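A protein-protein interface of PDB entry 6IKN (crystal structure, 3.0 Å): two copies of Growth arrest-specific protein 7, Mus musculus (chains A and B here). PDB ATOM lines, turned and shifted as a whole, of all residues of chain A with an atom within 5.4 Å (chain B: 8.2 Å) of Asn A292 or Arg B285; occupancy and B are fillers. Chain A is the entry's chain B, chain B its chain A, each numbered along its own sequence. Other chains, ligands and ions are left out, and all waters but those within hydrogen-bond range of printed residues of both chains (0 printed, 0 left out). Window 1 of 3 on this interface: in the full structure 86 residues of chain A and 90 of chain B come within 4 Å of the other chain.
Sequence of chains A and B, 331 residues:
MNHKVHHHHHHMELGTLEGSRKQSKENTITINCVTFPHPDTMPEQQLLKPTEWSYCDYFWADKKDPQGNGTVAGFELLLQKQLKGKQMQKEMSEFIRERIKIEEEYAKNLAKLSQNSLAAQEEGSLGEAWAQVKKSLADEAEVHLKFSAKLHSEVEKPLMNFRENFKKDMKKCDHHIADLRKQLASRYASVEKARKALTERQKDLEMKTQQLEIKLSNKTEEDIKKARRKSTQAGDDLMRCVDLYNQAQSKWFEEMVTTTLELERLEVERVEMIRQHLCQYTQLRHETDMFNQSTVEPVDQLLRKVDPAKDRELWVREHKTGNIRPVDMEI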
ATOM      1  N   GLU A 140      30.869  -0.677  10.055  1.00  0.00           N
ATOM      2  CA  GLU A 140      30.549  -0.491  11.470  1.00  0.00           C
ATOM      3  C   GLU A 140      31.811  -0.179  12.270  1.00  0.00           C
ATOM      4  O   GLU A 140      31.829   0.750  13.091  1.00  0.00           O
ATOM      5  CB  GLU A 140      29.863  -1.728  12.055  1.00  0.00           C
ATOM      6  CG  GLU A 140      28.516  -2.061  11.447  1.00  0.00           C
ATOM      7  CD  GLU A 140      27.916  -3.321  12.041  1.00  0.00           C
ATOM      8  OE1 GLU A 140      27.283  -4.094  11.292  1.00  0.00           O
ATOM      9  OE2 GLU A 140      28.072  -3.533  13.262  1.00  0.00           O
ATOM     10  N   VAL A 143      32.928   3.306  11.759  1.00  0.00           N
ATOM     11  CA  VAL A 143      31.984   4.197  12.430  1.00  0.00           C
ATOM     12  C   VAL A 143      32.327   4.329  13.916  1.00  0.00           C
ATOM     13  O   VAL A 143      32.450   5.444  14.434  1.00  0.00           O
ATOM     14  CB  VAL A 143      30.528   3.709  12.267  1.00  0.00           C
ATOM     15  CG1 VAL A 143      29.638   4.289  13.359  1.00  0.00           C
ATOM     16  CG2 VAL A 143      29.994   4.094  10.897  1.00  0.00           C
ATOM     17  N   HIS A 144      32.510   3.195  14.593  1.00  0.00           N
ATOM     18  CA  HIS A 144      32.830   3.217  16.020  1.00  0.00           C
ATOM     19  C   HIS A 144      34.193   3.853  16.302  1.00  0.00           C
ATOM     20  O   HIS A 144      34.370   4.535  17.320  1.00  0.00           O
ATOM     21  CB  HIS A 144      32.778   1.808  16.607  1.00  0.00           C
ATOM     22  CG  HIS A 144      31.392   1.321  16.879  1.00  0.00           C
ATOM     23  ND1 HIS A 144      30.848   1.295  18.149  1.00  0.00           N
ATOM     24  CD2 HIS A 144      30.431   0.844  16.054  1.00  0.00           C
ATOM     25  CE1 HIS A 144      29.619   0.824  18.090  1.00  0.00           C
ATOM     26  NE2 HIS A 144      29.339   0.541  16.827  1.00  0.00           N
ATOM     27  N   GLU A 287      23.801   9.901  17.456  1.00  0.00           N
ATOM     28  CA  GLU A 287      24.079   9.984  16.028  1.00  0.00           C
ATOM     29  C   GLU A 287      24.973   8.832  15.570  1.00  0.00           C
ATOM     30  O   GLU A 287      24.893   8.394  14.420  1.00  0.00           O
ATOM     31  CB  GLU A 287      24.714  11.333  15.680  1.00  0.00           C
ATOM     32  CG  GLU A 287      26.230  11.380  15.802  1.00  0.00           C
ATOM     33  CD  GLU A 287      26.790  12.768  15.557  1.00  0.00           C
ATOM     34  OE1 GLU A 287      26.017  13.745  15.656  1.00  0.00           O
ATOM     35  OE2 GLU A 287      28.001  12.881  15.272  1.00  0.00           O
ATOM     36  N   THR A 288      25.801   8.324  16.478  1.00  0.00           N
ATOM     37  CA  THR A 288      26.666   7.195  16.167  1.00  0.00           C
ATOM     38  C   THR A 288      25.826   5.944  15.973  1.00  0.00           C
ATOM     39  O   THR A 288      26.099   5.132  15.091  1.00  0.00           O
ATOM     40  CB  THR A 288      27.718   6.958  17.271  1.00  0.00           C
ATOM     41  OG1 THR A 288      28.701   8.000  17.221  1.00  0.00           O
ATOM     42  CG2 THR A 288      28.401   5.605  17.100  1.00  0.00           C
ATOM     43  N   ASP A 289      24.790   5.792  16.791  1.00  0.00           N
ATOM     44  CA  ASP A 289      23.904   4.644  16.640  1.00  0.00           C
ATOM     45  C   ASP A 289      23.045   4.770  15.383  1.00  0.00           C
ATOM     46  O   ASP A 289      22.703   3.762  14.757  1.00  0.00           O
ATOM     47  CB  ASP A 289      23.025   4.468  17.877  1.00  0.00           C
ATOM     48  CG  ASP A 289      23.742   3.735  18.995  1.00  0.00           C
ATOM     49  OD1 ASP A 289      24.637   2.913  18.690  1.00  0.00           O
ATOM     50  OD2 ASP A 289      23.411   3.975  20.175  1.00  0.00           O
ATOM     51  N   MET A 290      22.708   5.999  14.999  1.00  0.00           N
ATOM     52  CA  MET A 290      22.027   6.194  13.717  1.00  0.00           C
ATOM     53  C   MET A 290      22.924   5.763  12.552  1.00  0.00           C
ATOM     54  O   MET A 290      22.524   4.944  11.708  1.00  0.00           O
ATOM     55  CB  MET A 290      21.592   7.649  13.542  1.00  0.00           C
ATOM     56  CG  MET A 290      20.461   8.062  14.471  1.00  0.00           C
ATOM     57  SD  MET A 290      18.848   6.979  14.248  1.00  0.00           S
ATOM     58  CE  MET A 290      18.000   7.969  12.795  1.00  0.00           C
ATOM     59  N   PHE A 291      24.138   6.313  12.520  1.00  0.00           N
ATOM     60  CA  PHE A 291      25.121   5.965  11.496  1.00  0.00           C
ATOM     61  C   PHE A 291      25.322   4.459  11.421  1.00  0.00           C
ATOM     62  O   PHE A 291      25.315   3.875  10.338  1.00  0.00           O
ATOM     63  CB  PHE A 291      26.460   6.652  11.775  1.00  0.00           C
ATOM     64  CG  PHE A 291      26.427   8.142  11.595  1.00  0.00           C
ATOM     65  CD1 PHE A 291      25.557   8.720  10.684  1.00  0.00           C
ATOM     66  CD2 PHE A 291      27.264   8.965  12.332  1.00  0.00           C
ATOM     67  CE1 PHE A 291      25.521  10.091  10.511  1.00  0.00           C
ATOM     68  CE2 PHE A 291      27.232  10.339  12.162  1.00  0.00           C
ATOM     69  CZ  PHE A 291      26.360  10.902  11.250  1.00  0.00           C
ATOM     70  N   ASN A 292      25.472   3.838  12.585  1.00  0.00           N
ATOM     71  CA  ASN A 292      25.682   2.400  12.680  1.00  0.00           C
ATOM     72  C   ASN A 292      24.515   1.617  12.100  1.00  0.00           C
ATOM     73  O   ASN A 292      24.706   0.675  11.334  1.00  0.00           O
ATOM     74  CB  ASN A 292      25.905   1.998  14.137  1.00  0.00           C
ATOM     75  CG  ASN A 292      26.705   0.719  14.270  1.00  0.00           C
ATOM     76  OD1 ASN A 292      26.186  -0.305  14.711  1.00  0.00           O
ATOM     77  ND2 ASN A 292      27.976   0.768  13.877  1.00  0.00           N
ATOM     78  N   GLN A 293      23.303   2.017  12.468  1.00  0.00           N
ATOM     79  CA  GLN A 293      22.097   1.380  11.949  1.00  0.00           C
ATOM     80  C   GLN A 293      22.004   1.494  10.431  1.00  0.00           C
ATOM     81  O   GLN A 293      21.462   0.614   9.767  1.00  0.00           O
ATOM     82  CB  GLN A 293      20.854   1.983  12.598  1.00  0.00           C
ATOM     83  CG  GLN A 293      19.576   1.243  12.275  1.00  0.00           C
ATOM     84  CD  GLN A 293      18.353   1.981  12.760  1.00  0.00           C
ATOM     85  OE1 GLN A 293      18.431   3.155  13.126  1.00  0.00           O
ATOM     86  NE2 GLN A 293      17.214   1.299  12.776  1.00  0.00           N
ATOM     87  N   SER A 294      22.518   2.591   9.884  1.00  0.00           N
ATOM     88  CA  SER A 294      22.419   2.826   8.444  1.00  0.00           C
ATOM     89  C   SER A 294      23.327   1.936   7.580  1.00  0.00           C
ATOM     90  O   SER A 294      23.249   1.986   6.354  1.00  0.00           O
ATOM     91  CB  SER A 294      22.725   4.295   8.139  1.00  0.00           C
ATOM     92  OG  SER A 294      24.118   4.508   7.978  1.00  0.00           O
ATOM     93  N   THR A 295      24.175   1.121   8.202  1.00  0.00           N
ATOM     94  CA  THR A 295      25.160   0.346   7.441  1.00  0.00           C
ATOM     95  C   THR A 295      24.666  -0.995   6.892  1.00  0.00           C
ATOM     96  O   THR A 295      25.330  -1.604   6.054  1.00  0.00           O
ATOM     97  CB  THR A 295      26.424   0.071   8.284  1.00  0.00           C
ATOM     98  OG1 THR A 295      26.090  -0.749   9.411  1.00  0.00           O
ATOM     99  CG2 THR A 295      27.033   1.378   8.767  1.00  0.00           C
ATOM    100  N   VAL A 296      23.510  -1.459   7.352  1.00  0.00           N
ATOM    101  CA  VAL A 296      22.991  -2.742   6.894  1.00  0.00           C
ATOM    102  C   VAL A 296      22.068  -2.596   5.686  1.00  0.00           C
ATOM    103  O   VAL A 296      21.727  -3.581   5.031  1.00  0.00           O
ATOM    104  CB  VAL A 296      22.251  -3.470   8.025  1.00  0.00           C
ATOM    105  CG1 VAL A 296      23.228  -3.875   9.118  1.00  0.00           C
ATOM    106  CG2 VAL A 296      21.150  -2.593   8.584  1.00  0.00           C
ATOM    107  N   ARG B  99      31.247 -13.212  15.437  1.00  0.00           N
ATOM    108  CA  ARG B  99      30.537 -11.974  15.762  1.00  0.00           C
ATOM    109  C   ARG B  99      29.972 -12.003  17.187  1.00  0.00           C
ATOM    110  O   ARG B  99      30.104 -11.030  17.937  1.00  0.00           O
ATOM    111  CB  ARG B  99      29.419 -11.704  14.756  1.00  0.00           C
ATOM    112  CG  ARG B  99      28.466 -10.600  15.190  1.00  0.00           C
ATOM    113  CD  ARG B  99      29.072  -9.218  15.033  1.00  0.00           C
ATOM    114  NE  ARG B  99      28.328  -8.395  14.086  1.00  0.00           N
ATOM    115  CZ  ARG B  99      28.215  -7.073  14.170  1.00  0.00           C
ATOM    116  NH1 ARG B  99      28.795  -6.416  15.167  1.00  0.00           N
ATOM    117  NH2 ARG B  99      27.516  -6.408  13.262  1.00  0.00           N
ATOM    118  N   GLU B 103      30.825  -9.405  20.262  1.00  0.00           N
ATOM    119  CA  GLU B 103      29.774  -8.678  20.963  1.00  0.00           C
ATOM    120  C   GLU B 103      29.799  -8.972  22.459  1.00  0.00           C
ATOM    121  O   GLU B 103      29.579  -8.080  23.278  1.00  0.00           O
ATOM    122  CB  GLU B 103      28.401  -9.022  20.385  1.00  0.00           C
ATOM    123  CG  GLU B 103      28.204  -8.571  18.947  1.00  0.00           C
ATOM    124  CD  GLU B 103      28.285  -7.064  18.786  1.00  0.00           C
ATOM    125  OE1 GLU B 103      27.901  -6.338  19.726  1.00  0.00           O
ATOM    126  OE2 GLU B 103      28.737  -6.605  17.715  1.00  0.00           O
ATOM    127  N   VAL B 143      21.851  -4.584  26.107  1.00  0.00           N
ATOM    128  CA  VAL B 143      21.370  -4.569  24.724  1.00  0.00           C
ATOM    129  C   VAL B 143      22.207  -5.452  23.793  1.00  0.00           C
ATOM    130  O   VAL B 143      21.668  -6.298  23.075  1.00  0.00           O
ATOM    131  CB  VAL B 143      21.346  -3.127  24.165  1.00  0.00           C
ATOM    132  CG1 VAL B 143      21.385  -3.133  22.642  1.00  0.00           C
ATOM    133  CG2 VAL B 143      20.112  -2.393  24.659  1.00  0.00           C
ATOM    134  N   HIS B 144      23.522  -5.250  23.817  1.00  0.00           N
ATOM    135  CA  HIS B 144      24.443  -5.993  22.960  1.00  0.00           C
ATOM    136  C   HIS B 144      24.523  -7.476  23.320  1.00  0.00           C
ATOM    137  O   HIS B 144      24.647  -8.333  22.440  1.00  0.00           O
ATOM    138  CB  HIS B 144      25.833  -5.363  23.025  1.00  0.00           C
ATOM    139  CG  HIS B 144      25.958  -4.098  22.233  1.00  0.00           C
ATOM    140  ND1 HIS B 144      26.577  -4.046  21.005  1.00  0.00           N
ATOM    141  CD2 HIS B 144      25.535  -2.839  22.500  1.00  0.00           C
ATOM    142  CE1 HIS B 144      26.535  -2.804  20.546  1.00  0.00           C
ATOM    143  NE2 HIS B 144      25.909  -2.055  21.433  1.00  0.00           N
ATOM    144  N   PHE B 147      21.563  -8.988  21.984  1.00  0.00           N
ATOM    145  CA  PHE B 147      21.826  -9.070  20.551  1.00  0.00           C
ATOM    146  C   PHE B 147      22.582 -10.341  20.185  1.00  0.00           C
ATOM    147  O   PHE B 147      22.198 -11.053  19.260  1.00  0.00           O
ATOM    148  CB  PHE B 147      22.610  -7.844  20.081  1.00  0.00           C
ATOM    149  CG  PHE B 147      23.146  -7.964  18.683  1.00  0.00           C
ATOM    150  CD1 PHE B 147      22.299  -8.212  17.615  1.00  0.00           C
ATOM    151  CD2 PHE B 147      24.500  -7.812  18.435  1.00  0.00           C
ATOM    152  CE1 PHE B 147      22.794  -8.316  16.328  1.00  0.00           C
ATOM    153  CE2 PHE B 147      25.000  -7.914  17.152  1.00  0.00           C
ATOM    154  CZ  PHE B 147      24.145  -8.166  16.096  1.00  0.00           C
ATOM    155  N   LEU B 151      21.475 -13.570  18.040  1.00  0.00           N
ATOM    156  CA  LEU B 151      22.313 -14.057  16.946  1.00  0.00           C
ATOM    157  C   LEU B 151      22.483 -15.568  17.036  1.00  0.00           C
ATOM    158  O   LEU B 151      22.345 -16.276  16.042  1.00  0.00           O
ATOM    159  CB  LEU B 151      23.686 -13.384  16.958  1.00  0.00           C
ATOM    160  CG  LEU B 151      23.795 -11.995  16.333  1.00  0.00           C
ATOM    161  CD1 LEU B 151      25.251 -11.594  16.203  1.00  0.00           C
ATOM    162  CD2 LEU B 151      23.116 -11.980  14.974  1.00  0.00           C
ATOM    163  N   LEU B 278      19.747 -14.420   6.891  1.00  0.00           N
ATOM    164  CA  LEU B 278      20.553 -13.210   6.772  1.00  0.00           C
ATOM    165  C   LEU B 278      19.664 -11.977   6.933  1.00  0.00           C
ATOM    166  O   LEU B 278      20.078 -10.965   7.516  1.00  0.00           O
ATOM    167  CB  LEU B 278      21.300 -13.174   5.438  1.00  0.00           C
ATOM    168  CG  LEU B 278      22.432 -14.196   5.305  1.00  0.00           C
ATOM    169  CD1 LEU B 278      23.287 -13.894   4.086  1.00  0.00           C
ATOM    170  CD2 LEU B 278      23.287 -14.233   6.568  1.00  0.00           C
ATOM    171  N   CYS B 279      18.435 -12.065   6.430  1.00  0.00           N
ATOM    172  CA  CYS B 279      17.458 -11.009   6.671  1.00  0.00           C
ATOM    173  C   CYS B 279      17.180 -10.881   8.168  1.00  0.00           C
ATOM    174  O   CYS B 279      17.040  -9.767   8.696  1.00  0.00           O
ATOM    175  CB  CYS B 279      16.160 -11.287   5.915  1.00  0.00           C
ATOM    176  SG  CYS B 279      16.026 -10.446   4.327  1.00  0.00           S
ATOM    177  N   GLN B 280      17.125 -12.024   8.849  1.00  0.00           N
ATOM    178  CA  GLN B 280      16.980 -12.041  10.307  1.00  0.00           C
ATOM    179  C   GLN B 280      18.133 -11.283  10.963  1.00  0.00           C
ATOM    180  O   GLN B 280      17.917 -10.443  11.847  1.00  0.00           O
ATOM    181  CB  GLN B 280      16.910 -13.475  10.831  1.00  0.00           C
ATOM    182  CG  GLN B 280      15.578 -13.821  11.478  1.00  0.00           C
ATOM    183  CD  GLN B 280      15.184 -15.268  11.263  1.00  0.00           C
ATOM    184  OE1 GLN B 280      15.907 -16.187  11.650  1.00  0.00           O
ATOM    185  NE2 GLN B 280      14.031 -15.479  10.638  1.00  0.00           N
ATOM    186  N   TYR B 281      19.353 -11.601  10.538  1.00  0.00           N
ATOM    187  CA  TYR B 281      20.543 -10.881  10.990  1.00  0.00           C
ATOM    188  C   TYR B 281      20.372  -9.371  10.846  1.00  0.00           C
ATOM    189  O   TYR B 281      20.645  -8.610  11.779  1.00  0.00           O
ATOM    190  CB  TYR B 281      21.778 -11.349  10.214  1.00  0.00           C
ATOM    191  CG  TYR B 281      23.002 -10.473  10.392  1.00  0.00           C
ATOM    192  CD1 TYR B 281      23.827 -10.618  11.498  1.00  0.00           C
ATOM    193  CD2 TYR B 281      23.346  -9.520   9.439  1.00  0.00           C
ATOM    194  CE1 TYR B 281      24.947  -9.828  11.664  1.00  0.00           C
ATOM    195  CE2 TYR B 281      24.468  -8.725   9.596  1.00  0.00           C
ATOM    196  CZ  TYR B 281      25.264  -8.883  10.713  1.00  0.00           C
ATOM    197  OH  TYR B 281      26.382  -8.098  10.881  1.00  0.00           O
ATOM    198  N   THR B 282      19.906  -8.949   9.675  1.00  0.00           N
ATOM    199  CA  THR B 282      19.678  -7.532   9.411  1.00  0.00           C
ATOM    200  C   THR B 282      18.691  -6.917  10.407  1.00  0.00           C
ATOM    201  O   THR B 282      18.950  -5.843  10.976  1.00  0.00           O
ATOM    202  CB  THR B 282      19.160  -7.323   7.969  1.00  0.00           C
ATOM    203  OG1 THR B 282      20.269  -7.064   7.100  1.00  0.00           O
ATOM    204  CG2 THR B 282      18.181  -6.155   7.899  1.00  0.00           C
ATOM    205  N   GLN B 283      17.582  -7.618  10.638  1.00  0.00           N
ATOM    206  CA  GLN B 283      16.563  -7.150  11.575  1.00  0.00           C
ATOM    207  C   GLN B 283      17.149  -6.957  12.969  1.00  0.00           C
ATOM    208  O   GLN B 283      16.917  -5.930  13.627  1.00  0.00           O
ATOM    209  CB  GLN B 283      15.393  -8.132  11.632  1.00  0.00           C
ATOM    210  CG  GLN B 283      14.361  -7.795  12.693  1.00  0.00           C
ATOM    211  CD  GLN B 283      13.711  -6.443  12.462  1.00  0.00           C
ATOM    212  OE1 GLN B 283      13.370  -6.091  11.332  1.00  0.00           O
ATOM    213  NE2 GLN B 283      13.543  -5.675  13.534  1.00  0.00           N
ATOM    214  N   LEU B 284      17.922  -7.947  13.405  1.00  0.00           N
ATOM    215  CA  LEU B 284      18.560  -7.888  14.712  1.00  0.00           C
ATOM    216  C   LEU B 284      19.491  -6.687  14.803  1.00  0.00           C
ATOM    217  O   LEU B 284      19.501  -5.985  15.813  1.00  0.00           O
ATOM    218  CB  LEU B 284      19.320  -9.180  14.994  1.00  0.00           C
ATOM    219  CG  LEU B 284      18.401 -10.359  15.311  1.00  0.00           C
ATOM    220  CD1 LEU B 284      19.204 -11.606  15.656  1.00  0.00           C
ATOM    221  CD2 LEU B 284      17.448  -9.998  16.440  1.00  0.00           C
ATOM    222  N   ARG B 285      20.250  -6.443  13.737  1.00  0.00           N
ATOM    223  CA  ARG B 285      21.129  -5.277  13.671  1.00  0.00           C
ATOM    224  C   ARG B 285      20.347  -3.982  13.896  1.00  0.00           C
ATOM    225  O   ARG B 285      20.701  -3.160  14.759  1.00  0.00           O
ATOM    226  CB  ARG B 285      21.838  -5.231  12.314  1.00  0.00           C
ATOM    227  CG  ARG B 285      22.974  -6.230  12.139  1.00  0.00           C
ATOM    228  CD  ARG B 285      24.351  -5.623  12.416  1.00  0.00           C
ATOM    229  NE  ARG B 285      24.351  -4.612  13.469  1.00  0.00           N
ATOM    230  CZ  ARG B 285      24.409  -3.299  13.252  1.00  0.00           C
ATOM    231  NH1 ARG B 285      24.468  -2.826  12.013  1.00  0.00           N
ATOM    232  NH2 ARG B 285      24.405  -2.459  14.277  1.00  0.00           N
ATOM    233  N   HIS B 286      19.283  -3.813  13.114  1.00  0.00           N
ATOM    234  CA  HIS B 286      18.432  -2.628  13.211  1.00  0.00           C
ATOM    235  C   HIS B 286      17.882  -2.394  14.617  1.00  0.00           C
ATOM    236  O   HIS B 286      18.073  -1.317  15.208  1.00  0.00           O
ATOM    237  CB  HIS B 286      17.274  -2.725  12.221  1.00  0.00           C
ATOM    238  CG  HIS B 286      17.589  -2.152  10.877  1.00  0.00           C
ATOM    239  ND1 HIS B 286      17.746  -0.800  10.665  1.00  0.00           N
ATOM    240  CD2 HIS B 286      17.779  -2.746   9.676  1.00  0.00           C
ATOM    241  CE1 HIS B 286      18.025  -0.585   9.393  1.00  0.00           C
ATOM    242  NE2 HIS B 286      18.045  -1.748   8.768  1.00  0.00           N
ATOM    243  N   GLU B 287      17.195  -3.399  15.153  1.00  0.00           N
ATOM    244  CA  GLU B 287      16.532  -3.211  16.436  1.00  0.00           C
ATOM    245  C   GLU B 287      17.555  -3.068  17.562  1.00  0.00           C
ATOM    246  O   GLU B 287      17.287  -2.409  18.570  1.00  0.00           O
ATOM    247  CB  GLU B 287      15.563  -4.358  16.732  1.00  0.00           C
ATOM    248  CG  GLU B 287      16.176  -5.548  17.444  1.00  0.00           C
ATOM    249  CD  GLU B 287      15.188  -6.681  17.621  1.00  0.00           C
ATOM    250  OE1 GLU B 287      14.175  -6.704  16.892  1.00  0.00           O
ATOM    251  OE2 GLU B 287      15.421  -7.542  18.494  1.00  0.00           O
ATOM    252  N   THR B 288      18.731  -3.664  17.382  1.00  0.00           N
ATOM    253  CA  THR B 288      19.789  -3.540  18.377  1.00  0.00           C
ATOM    254  C   THR B 288      20.306  -2.115  18.408  1.00  0.00           C
ATOM    255  O   THR B 288      20.540  -1.559  19.480  1.00  0.00           O
ATOM    256  CB  THR B 288      20.961  -4.500  18.100  1.00  0.00           C
ATOM    257  OG1 THR B 288      20.563  -5.838  18.420  1.00  0.00           O
ATOM    258  CG2 THR B 288      22.178  -4.126  18.935  1.00  0.00           C
ATOM    259  N   ASP B 289      20.447  -1.504  17.236  1.00  0.00           N
ATOM    260  CA  ASP B 289      20.901  -0.117  17.213  1.00  0.00           C
ATOM    261  C   ASP B 289      19.828   0.841  17.724  1.00  0.00           C
ATOM    262  O   ASP B 289      20.148   1.876  18.312  1.00  0.00           O
ATOM    263  CB  ASP B 289      21.352   0.284  15.810  1.00  0.00           C
ATOM    264  CG  ASP B 289      22.779  -0.141  15.521  1.00  0.00           C
ATOM    265  OD1 ASP B 289      23.581  -0.217  16.477  1.00  0.00           O
ATOM    266  OD2 ASP B 289      23.099  -0.410  14.345  1.00  0.00           O
ATOM    267  N   MET B 290      18.559   0.495  17.528  1.00  0.00           N
ATOM    268  CA  MET B 290      17.491   1.324  18.089  1.00  0.00           C
ATOM    269  C   MET B 290      17.467   1.260  19.618  1.00  0.00           C
ATOM    270  O   MET B 290      17.513   2.301  20.295  1.00  0.00           O
ATOM    271  CB  MET B 290      16.133   0.917  17.517  1.00  0.00           C
ATOM    272  CG  MET B 290      15.865   1.497  16.140  1.00  0.00           C
ATOM    273  SD  MET B 290      16.640   3.282  15.944  1.00  0.00           S
ATOM    274  CE  MET B 290      15.056   4.243  15.338  1.00  0.00           C
ATOM    275  N   PHE B 291      17.391   0.043  20.156  1.00  0.00           N
ATOM    276  CA  PHE B 291      17.480  -0.166  21.600  1.00  0.00           C
ATOM    277  C   PHE B 291      18.699   0.537  22.179  1.00  0.00           C
ATOM    278  O   PHE B 291      18.612   1.182  23.221  1.00  0.00           O
ATOM    279  CB  PHE B 291      17.530  -1.657  21.940  1.00  0.00           C
ATOM    280  CG  PHE B 291      16.240  -2.382  21.689  1.00  0.00           C
ATOM    281  CD1 PHE B 291      15.027  -1.719  21.788  1.00  0.00           C
ATOM    282  CD2 PHE B 291      16.238  -3.729  21.362  1.00  0.00           C
ATOM    283  CE1 PHE B 291      13.837  -2.384  21.561  1.00  0.00           C
ATOM    284  CE2 PHE B 291      15.051  -4.399  21.134  1.00  0.00           C
ATOM    285  CZ  PHE B 291      13.850  -3.726  21.233  1.00  0.00           C
ATOM    286  N   ASN B 292      19.835   0.404  21.501  1.00  0.00           N
ATOM    287  CA  ASN B 292      21.060   1.047  21.952  1.00  0.00           C
ATOM    288  C   ASN B 292      20.911   2.561  21.998  1.00  0.00           C
ATOM    289  O   ASN B 292      21.315   3.201  22.968  1.00  0.00           O
ATOM    290  CB  ASN B 292      22.240   0.671  21.057  1.00  0.00           C
ATOM    291  CG  ASN B 292      23.570   0.781  21.778  1.00  0.00           C
ATOM    292  OD1 ASN B 292      24.391   1.638  21.463  1.00  0.00           O
ATOM    293  ND2 ASN B 292      23.780  -0.085  22.767  1.00  0.00           N
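Printed residues of chain A that touch a printed residue of chain B: Glu A140, Asp A289, Asn A292, Gln A293, Thr A295 and Val A296. Among the printed residues, Asp or Glu carboxylates within 4 Å of a Lys or Arg side-chain nitrogen of the other chain: Glu A140 with Arg B99 and Glu A140 with Arg B285.
Asn A292 touches just these residues of chain B: Arg B285 (2.8 Å) and Asp B289 (3.1 Å). Arg B285 touches four residues of chain A. Of the printed residues of chain A, Asp B289 touches Asp A289 (3.9 Å), Asn A292 (3.1 Å) and Gln A293 (3.1 Å). Printed residues of chain A within 4 Å of His B286: Gln A293 (3.0 Å) and Val A296 (3.2 Å). Of the printed residues of chain A, Met B290 touches Gln A293 (3.3 Å). Printed residues of chain B within 4 Å of Asp A289: Asp B289 and Asn B292. Printed residues of chain A within 4 Å of Arg B99: Glu A140 (2.9 Å). Val A143 touches none of the printed residues of chain B. The nearest printed residue of chain A that does not touch His B286 is Ser A294 (5.5 Å).
O of Asn A292 is in hydrogen-bond range of OG1 of Thr A295 (2.8 Å). The guanidinium group (NH2) of Arg B99 is in hydrogen-bond range of the side-chain hydroxyl (OH) of Tyr B281, at 3.1 Å. The guanidinium group (NH2) of Arg B285 lies within salt-bridge range of the side-chain carboxylate (OD2) of Asp B289, 2.4 Å away. The guanidinium group (NH1) of Arg B99 lies within salt-bridge range of the side-chain carboxylate (OE2) of Glu B103 (2.6 Å). NE2 of His B144 lies within hydrogen-bond range of ND2 of Asn B292. A ring nitrogen (NE2) of His A144 is in hydrogen-bond range of the side-chain amide nitrogen (ND2) of Asn A292 (3.3 Å).
Asp A289 touches its own counterpart, Asp B289. Asp A289 touches Asn B292, and with the chains exchanged Asn A292 touches Asp B289. Positions printed for both chains: 143, 144, 287, 288, 289, 290, 291 and 292. Of the 12 pairs that touch across the chains among the printed residues, 3 have their exchanged pair printed and touching as well.
The side-chain carboxylate of Asp B289 is in hydrogen-bond range of the backbone NH of Gln A293. The guanidinium group (NH2) of Arg B99 lies within salt-bridge range of the side-chain carboxylate (OE2) of Glu A140, 2.9 Å away. The side-chain carboxylate of Asp A289 sits close to the side-chain amide oxygen of Asn B292, at 2.8 Å. ND1 of His B286 is in hydrogen-bond range of NE2 of Gln A293 (3.0 Å). OD1 of Asn A292 lies within hydrogen-bond range of NH2 of Arg B285 (2.8 Å). OD2 of Asp B289 sits close to OD1 of Asn A292, at 3.1 Å. The guanidinium group (NH1) of Arg B285 lies within salt-bridge range of the side-chain carboxylate (OE1) of Glu A140 (3.2 Å). SD of Met B290 sits close to OE1 of Gln A293 (3.3 Å).
Asp A289 touches Asp B289 (O to CB, 3.9 Å). Thr A295 touches Arg B285 (OG1 to NH1, 3.7 Å). Val A296 touches Arg B285. Val A296 touches His B286.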
